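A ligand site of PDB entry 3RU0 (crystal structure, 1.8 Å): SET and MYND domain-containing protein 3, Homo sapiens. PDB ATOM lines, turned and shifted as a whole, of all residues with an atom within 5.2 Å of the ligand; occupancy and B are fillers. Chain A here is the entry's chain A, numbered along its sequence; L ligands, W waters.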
ATOM      1  N   ASN A  15       7.143   8.567 -28.622  1.00  0.00           N
ATOM      2  CA  ASN A  15       8.522   8.907 -28.303  1.00  0.00           C
ATOM      3  C   ASN A  15       9.182   8.049 -27.213  1.00  0.00           C
ATOM      4  O   ASN A  15      10.287   8.359 -26.772  1.00  0.00           O
ATOM      5  CB  ASN A  15       8.604  10.364 -27.861  1.00  0.00           C
ATOM      6  CG  ASN A  15       8.005  11.315 -28.874  1.00  0.00           C
ATOM      7  OD1 ASN A  15       7.041  12.018 -28.576  1.00  0.00           O
ATOM      8  ND2 ASN A  15       8.578  11.345 -30.081  1.00  0.00           N
ATOM      9  N   ARG A  16       8.510   6.992 -26.763  1.00  0.00           N
ATOM     10  CA  ARG A  16       9.080   6.233 -25.654  1.00  0.00           C
ATOM     11  C   ARG A  16       8.963   4.706 -25.855  1.00  0.00           C
ATOM     12  O   ARG A  16       8.789   3.959 -24.896  1.00  0.00           O
ATOM     13  CB  ARG A  16       8.498   6.717 -24.314  1.00  0.00           C
ATOM     14  CG  ARG A  16       6.984   6.834 -24.297  1.00  0.00           C
ATOM     15  CD  ARG A  16       6.378   6.881 -22.924  1.00  0.00           C
ATOM     16  NE  ARG A  16       6.421   8.214 -22.348  1.00  0.00           N
ATOM     17  CZ  ARG A  16       5.622   8.643 -21.370  1.00  0.00           C
ATOM     18  NH1 ARG A  16       4.696   7.835 -20.852  1.00  0.00           N
ATOM     19  NH2 ARG A  16       5.739   9.883 -20.915  1.00  0.00           N
ATOM     20  N   GLY A  17       9.068   4.266 -27.115  1.00  0.00           N
ATOM     21  CA  GLY A  17       9.034   2.840 -27.457  1.00  0.00           C
ATOM     22  C   GLY A  17       7.664   2.208 -27.360  1.00  0.00           C
ATOM     23  O   GLY A  17       6.655   2.830 -27.709  1.00  0.00           O
ATOM     24  N   ASN A  18       7.616   0.951 -26.944  1.00  0.00           N
ATOM     25  CA  ASN A  18       6.332   0.313 -26.725  1.00  0.00           C
ATOM     26  C   ASN A  18       5.824   0.686 -25.332  1.00  0.00           C
ATOM     27  O   ASN A  18       6.621   1.055 -24.463  1.00  0.00           O
ATOM     28  CB  ASN A  18       6.464  -1.188 -26.910  1.00  0.00           C
ATOM     29  CG  ASN A  18       6.940  -1.533 -28.297  1.00  0.00           C
ATOM     30  OD1 ASN A  18       6.406  -1.008 -29.265  1.00  0.00           O
ATOM     31  ND2 ASN A  18       7.975  -2.348 -28.400  1.00  0.00           N
ATOM     32  N   GLY A  19       4.522   0.631 -25.158  1.00  0.00           N
ATOM     33  CA  GLY A  19       3.912   0.869 -23.850  1.00  0.00           C
ATOM     34  C   GLY A  19       2.692  -0.035 -23.696  1.00  0.00           C
ATOM     35  O   GLY A  19       2.423  -0.844 -24.562  1.00  0.00           O
ATOM     36  N   TYR A 126       4.683  -9.627 -24.018  1.00  0.00           N
ATOM     37  CA  TYR A 126       6.024  -9.122 -24.362  1.00  0.00           C
ATOM     38  C   TYR A 126       6.992 -10.179 -23.878  1.00  0.00           C
ATOM     39  O   TYR A 126       6.830 -10.700 -22.775  1.00  0.00           O
ATOM     40  CB  TYR A 126       6.303  -7.836 -23.596  1.00  0.00           C
ATOM     41  CG  TYR A 126       7.121  -6.755 -24.300  1.00  0.00           C
ATOM     42  CD1 TYR A 126       6.814  -6.353 -25.613  1.00  0.00           C
ATOM     43  CD2 TYR A 126       8.113  -6.071 -23.608  1.00  0.00           C
ATOM     44  CE1 TYR A 126       7.503  -5.333 -26.202  1.00  0.00           C
ATOM     45  CE2 TYR A 126       8.816  -5.047 -24.198  1.00  0.00           C
ATOM     46  CZ  TYR A 126       8.485  -4.683 -25.504  1.00  0.00           C
ATOM     47  OH  TYR A 126       9.166  -3.669 -26.103  1.00  0.00           O
ATOM     48  N   ASP A 130      11.856  -9.196 -26.673  1.00  0.00           N
ATOM     49  CA  ASP A 130      11.298  -7.862 -26.942  1.00  0.00           C
ATOM     50  C   ASP A 130      11.892  -6.806 -26.018  1.00  0.00           C
ATOM     51  O   ASP A 130      11.870  -5.638 -26.335  1.00  0.00           O
ATOM     52  CB  ASP A 130       9.766  -7.859 -26.782  1.00  0.00           C
ATOM     53  CG  ASP A 130       9.032  -8.730 -27.798  1.00  0.00           C
ATOM     54  OD1 ASP A 130       9.371  -8.709 -28.976  1.00  0.00           O
ATOM     55  OD2 ASP A 130       8.072  -9.427 -27.432  1.00  0.00           O
ATOM     56  N   LEU A 131      12.427  -7.211 -24.862  1.00  0.00           N
ATOM     57  CA  LEU A 131      12.925  -6.230 -23.876  1.00  0.00           C
ATOM     58  C   LEU A 131      13.894  -5.213 -24.454  1.00  0.00           C
ATOM     59  O   LEU A 131      14.796  -5.538 -25.249  1.00  0.00           O
ATOM     60  CB  LEU A 131      13.556  -6.932 -22.679  1.00  0.00           C
ATOM     61  CG  LEU A 131      12.602  -7.819 -21.892  1.00  0.00           C
ATOM     62  CD1 LEU A 131      13.347  -8.479 -20.745  1.00  0.00           C
ATOM     63  CD2 LEU A 131      11.321  -7.037 -21.408  1.00  0.00           C
ATOM     64  N   GLU A 132      13.652  -3.960 -24.073  1.00  0.00           N
ATOM     65  CA  GLU A 132      14.484  -2.851 -24.497  1.00  0.00           C
ATOM     66  C   GLU A 132      15.847  -2.963 -23.831  1.00  0.00           C
ATOM     67  O   GLU A 132      15.943  -3.151 -22.616  1.00  0.00           O
ATOM     68  CB  GLU A 132      13.802  -1.540 -24.059  1.00  0.00           C
ATOM     69  CG  GLU A 132      14.609  -0.268 -24.384  1.00  0.00           C
ATOM     70  CD  GLU A 132      14.792  -0.084 -25.881  1.00  0.00           C
ATOM     71  OE1 GLU A 132      13.777   0.141 -26.576  1.00  0.00           O
ATOM     72  OE2 GLU A 132      15.948  -0.188 -26.358  1.00  0.00           O
ATOM     73  N   ASN A 134      18.414  -0.506 -24.686  1.00  0.00           N
ATOM     74  CA  ASN A 134      19.027   0.847 -24.796  1.00  0.00           C
ATOM     75  C   ASN A 134      20.515   0.815 -25.196  1.00  0.00           C
ATOM     76  O   ASN A 134      21.298   1.665 -24.762  1.00  0.00           O
ATOM     77  CB  ASN A 134      18.776   1.658 -23.490  1.00  0.00           C
ATOM     78  CG  ASN A 134      17.310   2.058 -23.308  1.00  0.00           C
ATOM     79  OD1 ASN A 134      16.744   1.907 -22.237  1.00  0.00           O
ATOM     80  ND2 ASN A 134      16.688   2.538 -24.371  1.00  0.00           N
ATOM     81  N   CYS A 182      17.513  -2.165 -17.288  1.00  0.00           N
ATOM     82  CA  CYS A 182      16.321  -1.355 -17.419  1.00  0.00           C
ATOM     83  C   CYS A 182      14.967  -2.111 -17.453  1.00  0.00           C
ATOM     84  O   CYS A 182      13.930  -1.498 -17.751  1.00  0.00           O
ATOM     85  CB  CYS A 182      16.461  -0.415 -18.607  1.00  0.00           C
ATOM     86  SG  CYS A 182      16.516  -1.259 -20.173  1.00  0.00           S
ATOM     87  N   ASN A 183      14.973  -3.413 -17.141  1.00  0.00           N
ATOM     88  CA  ASN A 183      13.759  -4.209 -17.064  1.00  0.00           C
ATOM     89  C   ASN A 183      13.667  -5.138 -15.829  1.00  0.00           C
ATOM     90  O   ASN A 183      12.799  -5.993 -15.783  1.00  0.00           O
ATOM     91  CB  ASN A 183      13.592  -5.039 -18.344  1.00  0.00           C
ATOM     92  CG  ASN A 183      13.496  -4.184 -19.601  1.00  0.00           C
ATOM     93  OD1 ASN A 183      12.454  -3.620 -19.889  1.00  0.00           O
ATOM     94  ND2 ASN A 183      14.584  -4.066 -20.319  1.00  0.00           N
ATOM     95  N   SER A 204       7.133  -5.492 -18.100  1.00  0.00           N
ATOM     96  CA  SER A 204       8.155  -4.547 -18.567  1.00  0.00           C
ATOM     97  C   SER A 204       7.700  -3.581 -19.654  1.00  0.00           C
ATOM     98  O   SER A 204       8.367  -2.606 -19.949  1.00  0.00           O
ATOM     99  CB  SER A 204       9.433  -5.264 -18.971  1.00  0.00           C
ATOM    100  OG  SER A 204      10.080  -5.751 -17.848  1.00  0.00           O
ATOM    101  N   LEU A 205       6.522  -3.823 -20.191  1.00  0.00           N
ATOM    102  CA  LEU A 205       5.935  -2.990 -21.188  1.00  0.00           C
ATOM    103  C   LEU A 205       5.531  -1.640 -20.603  1.00  0.00           C
ATOM    104  O   LEU A 205       5.543  -0.638 -21.307  1.00  0.00           O
ATOM    105  CB  LEU A 205       4.736  -3.719 -21.741  1.00  0.00           C
ATOM    106  CG  LEU A 205       4.205  -3.557 -23.127  1.00  0.00           C
ATOM    107  CD1 LEU A 205       5.287  -3.257 -24.180  1.00  0.00           C
ATOM    108  CD2 LEU A 205       3.451  -4.814 -23.393  1.00  0.00           C
ATOM    109  N   LEU A 206       5.234  -1.601 -19.299  1.00  0.00           N
ATOM    110  CA  LEU A 206       4.755  -0.351 -18.678  1.00  0.00           C
ATOM    111  C   LEU A 206       5.864   0.703 -18.615  1.00  0.00           C
ATOM    112  O   LEU A 206       6.939   0.474 -18.040  1.00  0.00           O
ATOM    113  CB  LEU A 206       4.184  -0.586 -17.295  1.00  0.00           C
ATOM    114  CG  LEU A 206       2.942  -1.458 -17.107  1.00  0.00           C
ATOM    115  CD1 LEU A 206       3.129  -2.353 -15.889  1.00  0.00           C
ATOM    116  CD2 LEU A 206       1.789  -0.648 -16.887  1.00  0.00           C
ATOM    117  N   ASN A 207       5.594   1.866 -19.234  1.00  0.00           N
ATOM    118  CA  ASN A 207       6.482   3.017 -19.075  1.00  0.00           C
ATOM    119  C   ASN A 207       6.389   3.648 -17.707  1.00  0.00           C
ATOM    120  O   ASN A 207       5.480   3.338 -16.956  1.00  0.00           O
ATOM    121  CB  ASN A 207       6.306   4.010 -20.248  1.00  0.00           C
ATOM    122  CG  ASN A 207       6.851   3.446 -21.551  1.00  0.00           C
ATOM    123  OD1 ASN A 207       7.982   2.935 -21.595  1.00  0.00           O
ATOM    124  ND2 ASN A 207       6.074   3.540 -22.593  1.00  0.00           N
ATOM    125  N   HIS A 208       7.360   4.488 -17.354  1.00  0.00           N
ATOM    126  CA  HIS A 208       7.436   5.127 -16.047  1.00  0.00           C
ATOM    127  C   HIS A 208       6.695   6.472 -15.972  1.00  0.00           C
ATOM    128  O   HIS A 208       6.678   7.232 -16.930  1.00  0.00           O
ATOM    129  CB  HIS A 208       8.937   5.419 -15.719  1.00  0.00           C
ATOM    130  CG  HIS A 208       9.134   6.213 -14.468  1.00  0.00           C
ATOM    131  ND1 HIS A 208       9.220   7.592 -14.475  1.00  0.00           N
ATOM    132  CD2 HIS A 208       9.219   5.838 -13.179  1.00  0.00           C
ATOM    133  CE1 HIS A 208       9.354   8.024 -13.240  1.00  0.00           C
ATOM    134  NE2 HIS A 208       9.339   6.985 -12.431  1.00  0.00           N
ATOM    135  N   SER A 209       6.142   6.758 -14.799  1.00  0.00           N
ATOM    136  CA  SER A 209       5.733   8.112 -14.405  1.00  0.00           C
ATOM    137  C   SER A 209       5.953   8.319 -12.919  1.00  0.00           C
ATOM    138  O   SER A 209       5.813   7.372 -12.140  1.00  0.00           O
ATOM    139  CB  SER A 209       4.251   8.337 -14.721  1.00  0.00           C
ATOM    140  OG  SER A 209       3.834   9.590 -14.196  1.00  0.00           O
ATOM    141  N   TYR A 241       8.861   3.712 -11.434  1.00  0.00           N
ATOM    142  CA  TYR A 241      10.045   2.852 -11.264  1.00  0.00           C
ATOM    143  C   TYR A 241      10.809   3.053  -9.930  1.00  0.00           C
ATOM    144  O   TYR A 241      11.627   2.218  -9.570  1.00  0.00           O
ATOM    145  CB  TYR A 241      11.051   3.011 -12.389  1.00  0.00           C
ATOM    146  CG  TYR A 241      10.598   2.592 -13.780  1.00  0.00           C
ATOM    147  CD1 TYR A 241       9.300   2.132 -14.018  1.00  0.00           C
ATOM    148  CD2 TYR A 241      11.463   2.743 -14.855  1.00  0.00           C
ATOM    149  CE1 TYR A 241       8.885   1.797 -15.312  1.00  0.00           C
ATOM    150  CE2 TYR A 241      11.080   2.380 -16.155  1.00  0.00           C
ATOM    151  CZ  TYR A 241       9.792   1.940 -16.382  1.00  0.00           C
ATOM    152  OH  TYR A 241       9.404   1.620 -17.655  1.00  0.00           O
ATOM    153  N   TYR A 259      17.972   4.136 -16.742  1.00  0.00           N
ATOM    154  CA  TYR A 259      16.938   3.886 -17.745  1.00  0.00           C
ATOM    155  C   TYR A 259      17.100   4.614 -19.071  1.00  0.00           C
ATOM    156  O   TYR A 259      16.267   4.478 -19.970  1.00  0.00           O
ATOM    157  CB  TYR A 259      15.554   4.160 -17.150  1.00  0.00           C
ATOM    158  CG  TYR A 259      15.186   3.198 -16.039  1.00  0.00           C
ATOM    159  CD1 TYR A 259      14.685   1.930 -16.339  1.00  0.00           C
ATOM    160  CD2 TYR A 259      15.317   3.571 -14.689  1.00  0.00           C
ATOM    161  CE1 TYR A 259      14.359   1.027 -15.331  1.00  0.00           C
ATOM    162  CE2 TYR A 259      14.994   2.667 -13.664  1.00  0.00           C
ATOM    163  CZ  TYR A 259      14.540   1.411 -13.982  1.00  0.00           C
ATOM    164  OH  TYR A 259      14.154   0.514 -13.011  1.00  0.00           O
ATOM    165  N   CYS A 260      18.171   5.362 -19.205  1.00  0.00           N
ATOM    166  CA  CYS A 260      18.438   6.116 -20.411  1.00  0.00           C
ATOM    167  C   CYS A 260      17.319   7.061 -20.896  1.00  0.00           C
ATOM    168  O   CYS A 260      17.046   7.135 -22.085  1.00  0.00           O
ATOM    169  CB  CYS A 260      18.919   5.158 -21.537  1.00  0.00           C
ATOM    170  SG  CYS A 260      20.475   4.386 -21.114  1.00  0.00           S
ATOM    171  N   PHE A 261      16.665   7.757 -19.973  1.00  0.00           N
ATOM    172  CA  PHE A 261      15.716   8.809 -20.385  1.00  0.00           C
ATOM    173  C   PHE A 261      15.678  10.000 -19.418  1.00  0.00           C
ATOM    174  O   PHE A 261      16.068   9.895 -18.272  1.00  0.00           O
ATOM    175  CB  PHE A 261      14.301   8.245 -20.687  1.00  0.00           C
ATOM    176  CG  PHE A 261      13.486   7.885 -19.466  1.00  0.00           C
ATOM    177  CD1 PHE A 261      12.589   8.806 -18.911  1.00  0.00           C
ATOM    178  CD2 PHE A 261      13.607   6.639 -18.882  1.00  0.00           C
ATOM    179  CE1 PHE A 261      11.823   8.474 -17.819  1.00  0.00           C
ATOM    180  CE2 PHE A 261      12.830   6.287 -17.755  1.00  0.00           C
ATOM    181  CZ  PHE A 261      11.937   7.229 -17.222  1.00  0.00           C
ATOM    182  N   GLU A 262      15.262  11.142 -19.940  1.00  0.00           N
ATOM    183  CA  GLU A 262      14.953  12.337 -19.137  1.00  0.00           C
ATOM    184  C   GLU A 262      13.476  12.325 -18.822  1.00  0.00           C
ATOM    185  O   GLU A 262      12.623  12.338 -19.729  1.00  0.00           O
ATOM    186  CB  GLU A 262      15.305  13.621 -19.913  1.00  0.00           C
ATOM    187  CG  GLU A 262      16.744  13.647 -20.484  1.00  0.00           C
ATOM    188  CD  GLU A 262      17.809  13.606 -19.401  1.00  0.00           C
ATOM    189  OE1 GLU A 262      18.801  12.867 -19.587  1.00  0.00           O
ATOM    190  OE2 GLU A 262      17.650  14.301 -18.371  1.00  0.00           O
ATOM    191  N   CYS A 263      13.146  12.271 -17.542  1.00  0.00           N
ATOM    192  CA  CYS A 263      11.744  12.299 -17.179  1.00  0.00           C
ATOM    193  C   CYS A 263      11.164  13.708 -17.324  1.00  0.00           C
ATOM    194  O   CYS A 263      11.645  14.634 -16.711  1.00  0.00           O
ATOM    195  CB  CYS A 263      11.496  11.805 -15.758  1.00  0.00           C
ATOM    196  SG  CYS A 263       9.775  11.500 -15.568  1.00  0.00           S
ATOM    197  N   ASP A 264      10.096  13.809 -18.105  1.00  0.00           N
ATOM    198  CA  ASP A 264       9.405  15.078 -18.410  1.00  0.00           C
ATOM    199  C   ASP A 264       8.025  15.098 -17.846  1.00  0.00           C
ATOM    200  O   ASP A 264       7.155  15.838 -18.326  1.00  0.00           O
ATOM    201  CB  ASP A 264       9.292  15.233 -19.946  1.00  0.00           C
ATOM    202  CG  ASP A 264       8.430  14.143 -20.603  1.00  0.00           C
ATOM    203  OD1 ASP A 264       7.979  13.186 -19.936  1.00  0.00           O
ATOM    204  OD2 ASP A 264       8.167  14.245 -21.821  1.00  0.00           O
HETATM  205  N1  LIG L   1       9.298   1.610 -23.608  1.00  0.00           N
HETATM  206  C1  LIG L   1       9.805   0.243 -23.298  1.00  0.00           C
HETATM  207  C2  LIG L   1       9.875  -0.763 -24.471  1.00  0.00           C
HETATM  208  O1  LIG L   1      10.101  -1.966 -24.280  1.00  0.00           O
HETATM  209  O2  LIG L   1       9.713  -0.373 -25.625  1.00  0.00           O
HETATM  210  C3  LIG L   1       8.959  -0.277 -22.087  1.00  0.00           C
HETATM  211  C4  LIG L   1       9.502   0.079 -20.678  1.00  0.00           C
HETATM  212  C5  LIG L   1      10.947  -0.443 -20.307  1.00  0.00           C
HETATM  213  N2  LIG L   1      10.848  -1.349 -19.117  1.00  0.00           N
HETATM  214  C6  LIG L   1      12.031   0.596 -19.908  1.00  0.00           C
HETATM  215  C7  LIG L   1      12.445   1.676 -20.944  1.00  0.00           C
HETATM  216  O3  LIG L   1      11.329   2.413 -21.528  1.00  0.00           O
HETATM  217  C8  LIG L   1      13.300   2.783 -20.354  1.00  0.00           C
HETATM  218  O4  LIG L   1      14.632   2.368 -20.166  1.00  0.00           O
HETATM  219  C9  LIG L   1      13.214   3.842 -21.427  1.00  0.00           C
HETATM  220  O5  LIG L   1      13.956   3.406 -22.566  1.00  0.00           O
HETATM  221  C10 LIG L   1      11.714   3.788 -21.720  1.00  0.00           C
HETATM  222  N3  LIG L   1      10.879   4.640 -20.867  1.00  0.00           N
HETATM  223  C11 LIG L   1      10.125   4.247 -19.780  1.00  0.00           C
HETATM  224  N4  LIG L   1       9.489   5.235 -19.237  1.00  0.00           N
HETATM  225  C12 LIG L   1       9.829   6.348 -20.020  1.00  0.00           C
HETATM  226  C13 LIG L   1       9.481   7.725 -19.961  1.00  0.00           C
HETATM  227  N5  LIG L   1       8.628   8.269 -19.051  1.00  0.00           N
HETATM  228  N6  LIG L   1       9.999   8.578 -20.895  1.00  0.00           N
HETATM  229  C14 LIG L   1      10.846   8.051 -21.809  1.00  0.00           C
HETATM  230  N7  LIG L   1      11.244   6.781 -21.963  1.00  0.00           N
HETATM  231  C15 LIG L   1      10.701   5.983 -21.023  1.00  0.00           C
HETATM  232  O   HOH W   1      11.830   2.308 -24.794  1.00  0.00           O
HETATM  233  O   HOH W   2      13.078   6.518 -24.052  1.00  0.00           O
HETATM  234  O   HOH W   3      15.391   5.574 -23.506  1.00  0.00           O
HETATM  235  O   HOH W   4       7.982  10.860 -18.226  1.00  0.00           O
HETATM  236  O   HOH W   5      11.400  -3.474 -22.483  1.00  0.00           O
HETATM  237  O   HOH W   6      11.354  -1.104 -27.563  1.00  0.00           O
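OH of Tyr 126 is in hydrogen-bond range of O1 of the ligand (2.7 Å).
The backbone carbonyl oxygen (O) of Tyr 259 sits at hydrogen-bond distance from an oxygen (O4) of the ligand.
The backbone carbonyl oxygen (O) of Arg 16 sits at hydrogen-bond distance from a nitrogen (N1) of the ligand.
The side-chain amide oxygen of Asn 207 lies within hydrogen-bond range of a nitrogen (N1) of the ligand (2.7 Å).
An oxygen (O2) of the ligand lies within hydrogen-bond range of the backbone NH of Asn 18 (2.8 Å).
O of Asn 18 lies within hydrogen-bond range of N1 of the ligand (2.9 Å).
OD1 of Asn 183 is in hydrogen-bond range of N2 of the ligand (2.9 Å).
O of Ser 204 sits at hydrogen-bond distance from N2 of the ligand (2.9 Å).
The backbone NH of His 208 lies within hydrogen-bond range of a nitrogen (N4) of the ligand (2.9 Å).
A nitrogen (N5) of the ligand is in hydrogen-bond range of the backbone carbonyl oxygen (O) of His 208 (3.1 Å).
OD1 of Asn 134 lies within hydrogen-bond range of O4 of the ligand (3.0 Å).
A nitrogen (N2) of the ligand sits at hydrogen-bond distance from the backbone carbonyl oxygen of Cys 182, at 3.4 Å.
The side-chain hydroxyl (OH) of Tyr 126 sits at hydrogen-bond distance from the side-chain amide nitrogen (ND2) of Asn 18, at 2.9 Å.
OH of Tyr 126 is in hydrogen-bond range of O of Asp 130, 3.4 Å away.
O of Tyr 259 lies close to OD1 of Asn 134 (3.5 Å).
The side-chain amide nitrogen (ND2) of Asn 207 is in hydrogen-bond range of the backbone carbonyl oxygen (O) of Asn 18 (3.2 Å).
A ring nitrogen (NE2) of His 208 lies close to the backbone NH (N) of Tyr 241 (3.5 Å).
The side-chain amide oxygen (OD1) of Asn 134 sits at hydrogen-bond distance from the side-chain sulfur (SG) of Cys 182 (3.8 Å).
The backbone NH of Asn 134 lies within hydrogen-bond range of the side-chain carboxylate of Glu 132, 3.0 Å away.
The side-chain sulfur of Cys 182 sits at hydrogen-bond distance from the backbone carbonyl oxygen of Glu 132, at 3.1 Å.
Gly 17 touches the ligand (C to O2, 3.7 Å).
Glu 132 touches the ligand.
Leu 205 touches the ligand (O to C3, 3.5 Å).
Leu 206 touches the ligand (O to C4, 3.7 Å).
Tyr 241 touches the ligand (OH to C4, 3.4 Å).
CE1 of Phe 261 touches C13 of the ligand, 3.3 Å away.
Hydrophobic or aromatic side chains that line the ligand: Tyr 126, His 208, Tyr 259 and Phe 261.
The nearest printed residue that does not touch the ligand is Asp 130 (4.6 Å).
Water W6 bridges an oxygen (O2) of the ligand and the side-chain carboxylate of Glu 132.
Water W5 lies within hydrogen-bond range of an oxygen (O1) of the ligand (2.7 Å), the backbone NH of Glu 132 (2.8 Å) and the side-chain amide oxygen of Asn 183 (2.8 Å).
Water W3 lies within hydrogen-bond range of O of Cys 260 (2.7 Å), O5 of the ligand (2.8 Å) and ND2 of Asn 134 (3.4 Å).
Water W4 lies within hydrogen-bond range of a nitrogen (N5) of the ligand and the side-chain carboxylate of Asp 264.
Water W1 lies within hydrogen-bond range of a nitrogen (N1) of the ligand, the side-chain carboxylate of Glu 132 and the backbone carbonyl oxygen of Arg 16.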
